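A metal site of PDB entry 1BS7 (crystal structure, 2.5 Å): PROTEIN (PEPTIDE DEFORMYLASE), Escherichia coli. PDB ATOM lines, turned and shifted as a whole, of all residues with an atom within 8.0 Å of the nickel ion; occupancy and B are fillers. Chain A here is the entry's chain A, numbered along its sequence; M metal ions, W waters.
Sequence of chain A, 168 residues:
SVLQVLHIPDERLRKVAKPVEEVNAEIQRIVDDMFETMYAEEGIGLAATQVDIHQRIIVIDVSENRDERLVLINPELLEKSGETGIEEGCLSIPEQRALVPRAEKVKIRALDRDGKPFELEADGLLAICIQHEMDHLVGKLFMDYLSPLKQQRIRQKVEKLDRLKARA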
ATOM      1  N   VAL A   5       0.531  19.779   1.531  1.00  0.00           N
ATOM      2  CA  VAL A   5      -0.483  20.336   2.426  1.00  0.00           C
ATOM      3  C   VAL A   5      -0.333  19.712   3.819  1.00  0.00           C
ATOM      4  O   VAL A   5      -0.292  18.486   3.946  1.00  0.00           O
ATOM      5  CB  VAL A   5      -1.913  20.072   1.918  1.00  0.00           C
ATOM      6  CG1 VAL A   5      -2.919  20.585   2.912  1.00  0.00           C
ATOM      7  CG2 VAL A   5      -2.132  20.771   0.586  1.00  0.00           C
ATOM      8  N   GLY A  45     -11.001  25.171  -1.919  1.00  0.00           N
ATOM      9  CA  GLY A  45     -10.339  26.306  -1.323  1.00  0.00           C
ATOM     10  C   GLY A  45      -8.982  25.875  -0.802  1.00  0.00           C
ATOM     11  O   GLY A  45      -8.782  24.711  -0.450  1.00  0.00           O
ATOM     12  N   LEU A  46      -8.045  26.811  -0.778  1.00  0.00           N
ATOM     13  CA  LEU A  46      -6.780  26.587  -0.103  1.00  0.00           C
ATOM     14  C   LEU A  46      -6.281  27.929   0.415  1.00  0.00           C
ATOM     15  O   LEU A  46      -6.449  28.947  -0.247  1.00  0.00           O
ATOM     16  CB  LEU A  46      -5.770  26.001  -1.081  1.00  0.00           C
ATOM     17  CG  LEU A  46      -4.545  25.289  -0.523  1.00  0.00           C
ATOM     18  CD1 LEU A  46      -4.899  23.950   0.105  1.00  0.00           C
ATOM     19  CD2 LEU A  46      -3.618  25.073  -1.701  1.00  0.00           C
ATOM     20  N   ALA A  47      -5.871  27.951   1.690  1.00  0.00           N
ATOM     21  CA  ALA A  47      -5.239  29.103   2.272  1.00  0.00           C
ATOM     22  C   ALA A  47      -3.738  28.867   2.300  1.00  0.00           C
ATOM     23  O   ALA A  47      -3.295  27.724   2.527  1.00  0.00           O
ATOM     24  CB  ALA A  47      -5.769  29.345   3.681  1.00  0.00           C
ATOM     25  N   GLN A  50      -1.888  26.656   4.863  1.00  0.00           N
ATOM     26  CA  GLN A  50      -1.973  25.213   4.740  1.00  0.00           C
ATOM     27  C   GLN A  50      -0.782  24.626   3.990  1.00  0.00           C
ATOM     28  O   GLN A  50      -0.502  23.420   4.085  1.00  0.00           O
ATOM     29  CB  GLN A  50      -3.239  24.820   4.005  1.00  0.00           C
ATOM     30  CG  GLN A  50      -4.485  24.794   4.862  1.00  0.00           C
ATOM     31  CD  GLN A  50      -5.730  24.463   4.043  1.00  0.00           C
ATOM     32  OE1 GLN A  50      -6.321  25.340   3.406  1.00  0.00           O
ATOM     33  NE2 GLN A  50      -6.097  23.189   4.012  1.00  0.00           N
ATOM     34  N   GLU A  88     -18.712  20.564   6.082  1.00  0.00           N
ATOM     35  CA  GLU A  88     -17.468  21.076   5.526  1.00  0.00           C
ATOM     36  C   GLU A  88     -16.363  20.046   5.583  1.00  0.00           C
ATOM     37  O   GLU A  88     -16.303  19.231   6.494  1.00  0.00           O
ATOM     38  CB  GLU A  88     -17.008  22.323   6.295  1.00  0.00           C
ATOM     39  CG  GLU A  88     -17.747  23.574   5.923  1.00  0.00           C
ATOM     40  CD  GLU A  88     -17.314  24.784   6.736  1.00  0.00           C
ATOM     41  OE1 GLU A  88     -16.109  24.922   7.032  1.00  0.00           O
ATOM     42  OE2 GLU A  88     -18.191  25.605   7.071  1.00  0.00           O
ATOM     43  N   GLY A  89     -15.461  20.132   4.620  1.00  0.00           N
ATOM     44  CA  GLY A  89     -14.207  19.406   4.740  1.00  0.00           C
ATOM     45  C   GLY A  89     -13.024  20.353   4.680  1.00  0.00           C
ATOM     46  O   GLY A  89     -13.190  21.584   4.631  1.00  0.00           O
ATOM     47  N   CYS A  90     -11.840  19.769   4.535  1.00  0.00           N
ATOM     48  CA  CYS A  90     -10.582  20.513   4.633  1.00  0.00           C
ATOM     49  C   CYS A  90      -9.463  19.573   4.209  1.00  0.00           C
ATOM     50  O   CYS A  90      -9.400  18.424   4.662  1.00  0.00           O
ATOM     51  CB  CYS A  90     -10.369  20.944   6.082  1.00  0.00           C
ATOM     52  SG  CYS A  90      -9.078  22.124   6.317  1.00  0.00           S
ATOM     53  N   LEU A  91      -8.585  20.052   3.321  1.00  0.00           N
ATOM     54  CA  LEU A  91      -7.471  19.221   2.873  1.00  0.00           C
ATOM     55  C   LEU A  91      -6.495  18.884   4.026  1.00  0.00           C
ATOM     56  O   LEU A  91      -5.777  17.892   3.964  1.00  0.00           O
ATOM     57  CB  LEU A  91      -6.739  19.913   1.710  1.00  0.00           C
ATOM     58  CG  LEU A  91      -7.524  20.061   0.403  1.00  0.00           C
ATOM     59  CD1 LEU A  91      -6.697  20.772  -0.677  1.00  0.00           C
ATOM     60  CD2 LEU A  91      -7.898  18.689  -0.083  1.00  0.00           C
ATOM     61  N   SER A  92      -6.529  19.692   5.097  1.00  0.00           N
ATOM     62  CA  SER A  92      -5.639  19.507   6.235  1.00  0.00           C
ATOM     63  C   SER A  92      -6.215  18.571   7.301  1.00  0.00           C
ATOM     64  O   SER A  92      -5.500  18.155   8.221  1.00  0.00           O
ATOM     65  CB  SER A  92      -5.342  20.859   6.860  1.00  0.00           C
ATOM     66  OG  SER A  92      -4.620  21.665   5.941  1.00  0.00           O
ATOM     67  N   ILE A  93      -7.516  18.309   7.205  1.00  0.00           N
ATOM     68  CA  ILE A  93      -8.202  17.369   8.090  1.00  0.00           C
ATOM     69  C   ILE A  93      -8.846  16.282   7.236  1.00  0.00           C
ATOM     70  O   ILE A  93     -10.044  16.364   6.919  1.00  0.00           O
ATOM     71  CB  ILE A  93      -9.304  18.060   8.908  1.00  0.00           C
ATOM     72  CG1 ILE A  93      -8.705  19.176   9.752  1.00  0.00           C
ATOM     73  CG2 ILE A  93      -9.969  17.049   9.826  1.00  0.00           C
ATOM     74  CD1 ILE A  93      -9.728  20.096  10.370  1.00  0.00           C
ATOM     75  N   ARG A 102     -21.942  29.150  10.073  1.00  0.00           N
ATOM     76  CA  ARG A 102     -21.347  30.182   9.265  1.00  0.00           C
ATOM     77  C   ARG A 102     -22.345  31.282   9.055  1.00  0.00           C
ATOM     78  O   ARG A 102     -23.535  31.069   9.214  1.00  0.00           O
ATOM     79  CB  ARG A 102     -20.956  29.627   7.902  1.00  0.00           C
ATOM     80  CG  ARG A 102     -19.885  28.567   7.903  1.00  0.00           C
ATOM     81  CD  ARG A 102     -18.549  29.092   8.362  1.00  0.00           C
ATOM     82  NE  ARG A 102     -17.544  28.032   8.295  1.00  0.00           N
ATOM     83  CZ  ARG A 102     -16.352  28.063   8.876  1.00  0.00           C
ATOM     84  NH1 ARG A 102     -15.925  29.160   9.480  1.00  0.00           N
ATOM     85  NH2 ARG A 102     -15.575  26.997   8.807  1.00  0.00           N
ATOM     86  N   CYS A 129     -17.327  29.062   2.127  1.00  0.00           N
ATOM     87  CA  CYS A 129     -16.001  28.814   1.588  1.00  0.00           C
ATOM     88  C   CYS A 129     -15.001  29.898   1.954  1.00  0.00           C
ATOM     89  O   CYS A 129     -13.901  29.627   2.396  1.00  0.00           O
ATOM     90  CB  CYS A 129     -16.126  28.716   0.084  1.00  0.00           C
ATOM     91  SG  CYS A 129     -15.190  27.426  -0.614  1.00  0.00           S
ATOM     92  N   HIS A 132     -14.395  29.847   5.815  1.00  0.00           N
ATOM     93  CA  HIS A 132     -13.544  28.722   6.148  1.00  0.00           C
ATOM     94  C   HIS A 132     -12.093  29.076   5.857  1.00  0.00           C
ATOM     95  O   HIS A 132     -11.228  28.891   6.703  1.00  0.00           O
ATOM     96  CB  HIS A 132     -13.968  27.517   5.312  1.00  0.00           C
ATOM     97  CG  HIS A 132     -13.091  26.311   5.472  1.00  0.00           C
ATOM     98  ND1 HIS A 132     -13.567  25.109   5.939  1.00  0.00           N
ATOM     99  CD2 HIS A 132     -11.803  26.082   5.127  1.00  0.00           C
ATOM    100  CE1 HIS A 132     -12.618  24.196   5.892  1.00  0.00           C
ATOM    101  NE2 HIS A 132     -11.529  24.766   5.393  1.00  0.00           N
ATOM    102  N   GLU A 133     -11.857  29.660   4.685  1.00  0.00           N
ATOM    103  CA  GLU A 133     -10.488  29.946   4.255  1.00  0.00           C
ATOM    104  C   GLU A 133      -9.870  31.082   5.065  1.00  0.00           C
ATOM    105  O   GLU A 133      -8.709  31.008   5.463  1.00  0.00           O
ATOM    106  CB  GLU A 133     -10.457  30.310   2.759  1.00  0.00           C
ATOM    107  CG  GLU A 133     -10.738  29.143   1.801  1.00  0.00           C
ATOM    108  CD  GLU A 133     -10.066  27.832   2.216  1.00  0.00           C
ATOM    109  OE1 GLU A 133      -8.940  27.845   2.779  1.00  0.00           O
ATOM    110  OE2 GLU A 133     -10.641  26.766   1.922  1.00  0.00           O
ATOM    111  N   ASP A 135     -10.518  31.866   8.074  1.00  0.00           N
ATOM    112  CA  ASP A 135     -10.203  31.281   9.381  1.00  0.00           C
ATOM    113  C   ASP A 135      -8.808  30.671   9.404  1.00  0.00           C
ATOM    114  O   ASP A 135      -8.199  30.600  10.445  1.00  0.00           O
ATOM    115  CB  ASP A 135     -11.198  30.179   9.721  1.00  0.00           C
ATOM    116  CG  ASP A 135     -12.398  30.686  10.449  1.00  0.00           C
ATOM    117  OD1 ASP A 135     -12.496  31.911  10.683  1.00  0.00           O
ATOM    118  OD2 ASP A 135     -13.232  29.838  10.797  1.00  0.00           O
ATOM    119  N   HIS A 136      -8.391  30.077   8.300  1.00  0.00           N
ATOM    120  CA  HIS A 136      -7.078  29.451   8.238  1.00  0.00           C
ATOM    121  C   HIS A 136      -6.026  30.512   8.478  1.00  0.00           C
ATOM    122  O   HIS A 136      -5.095  30.289   9.247  1.00  0.00           O
ATOM    123  CB  HIS A 136      -6.833  28.835   6.853  1.00  0.00           C
ATOM    124  CG  HIS A 136      -7.391  27.457   6.684  1.00  0.00           C
ATOM    125  ND1 HIS A 136      -7.016  26.388   7.473  1.00  0.00           N
ATOM    126  CD2 HIS A 136      -8.272  26.951   5.777  1.00  0.00           C
ATOM    127  CE1 HIS A 136      -7.647  25.300   7.067  1.00  0.00           C
ATOM    128  NE2 HIS A 136      -8.408  25.615   6.040  1.00  0.00           N
ATOM    129  N   LYS A 140      -7.384  29.301  12.715  1.00  0.00           N
ATOM    130  CA  LYS A 140      -8.634  28.654  13.072  1.00  0.00           C
ATOM    131  C   LYS A 140      -8.960  27.493  12.114  1.00  0.00           C
ATOM    132  O   LYS A 140      -8.957  27.661  10.891  1.00  0.00           O
ATOM    133  CB  LYS A 140      -9.757  29.669  12.988  1.00  0.00           C
ATOM    134  CG  LYS A 140     -10.057  30.358  14.255  1.00  0.00           C
ATOM    135  CD  LYS A 140     -10.790  29.413  15.160  1.00  0.00           C
ATOM    136  CE  LYS A 140     -12.251  29.274  14.736  1.00  0.00           C
ATOM    137  NZ  LYS A 140     -13.011  30.560  14.965  1.00  0.00           N
ATOM    138  N   LEU A 141      -9.313  26.340  12.690  1.00  0.00           N
ATOM    139  CA  LEU A 141      -9.785  25.208  11.909  1.00  0.00           C
ATOM    140  C   LEU A 141     -11.270  24.998  12.214  1.00  0.00           C
ATOM    141  O   LEU A 141     -11.765  25.478  13.217  1.00  0.00           O
ATOM    142  CB  LEU A 141      -8.993  23.955  12.249  1.00  0.00           C
ATOM    143  CG  LEU A 141      -7.465  24.074  12.165  1.00  0.00           C
ATOM    144  CD1 LEU A 141      -6.843  22.904  12.833  1.00  0.00           C
ATOM    145  CD2 LEU A 141      -7.032  24.156  10.721  1.00  0.00           C
ATOM    146  N   PHE A 142     -11.976  24.307  11.322  1.00  0.00           N
ATOM    147  CA  PHE A 142     -13.416  24.139  11.497  1.00  0.00           C
ATOM    148  C   PHE A 142     -13.773  23.241  12.690  1.00  0.00           C
ATOM    149  O   PHE A 142     -14.852  23.389  13.252  1.00  0.00           O
ATOM    150  CB  PHE A 142     -14.076  23.631  10.193  1.00  0.00           C
ATOM    151  CG  PHE A 142     -13.885  22.161   9.916  1.00  0.00           C
ATOM    152  CD1 PHE A 142     -14.439  21.190  10.770  1.00  0.00           C
ATOM    153  CD2 PHE A 142     -13.317  21.747   8.726  1.00  0.00           C
ATOM    154  CE1 PHE A 142     -14.425  19.843  10.436  1.00  0.00           C
ATOM    155  CE2 PHE A 142     -13.303  20.386   8.381  1.00  0.00           C
ATOM    156  CZ  PHE A 142     -13.866  19.435   9.248  1.00  0.00           C
HETATM  157 NI    NI M   1      -9.703  23.798   5.253  1.00  0.00          NI
HETATM  158  O   HOH W   1      -8.952  25.078   3.223  1.00  0.00           O
HETATM  159  O   HOH W   2     -10.396  23.642   8.411  1.00  0.00           O
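A ring nitrogen (ND1) of His 132 is in hydrogen-bond range of the side-chain carboxylate of Glu 88. N of Ser 92 sits close to SG of Cys 90, 3.7 Å away. A ring nitrogen (NE2) of His 136 lies close to the side-chain amide oxygen of Gln 50 (3.4 Å). NE2 of Gln 50 is in hydrogen-bond range of OG of Ser 92. The backbone NH (N) of Ala 47 is in hydrogen-bond range of the side-chain amide oxygen (OE1) of Gln 50 (3.2 Å).
NE2 of Gln 50 touches the nickel ion, 3.9 Å away. Within 4 Å of the nickel ion: Gln 50, Cys 90, His 132 and His 136.
The nickel ion is bound by NE2 of His 132 (2.1 Å), SG of Cys 90 (2.1 Å), NE2 of His 136 (2.4 Å) and water W1 (2.5 Å). The nickel ion has four donor atoms within binding distance.
Water W1 lies within hydrogen-bond range of the side-chain amide oxygen (OE1) of Gln 50 and the side-chain carboxylate (OE2) of Glu 133.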
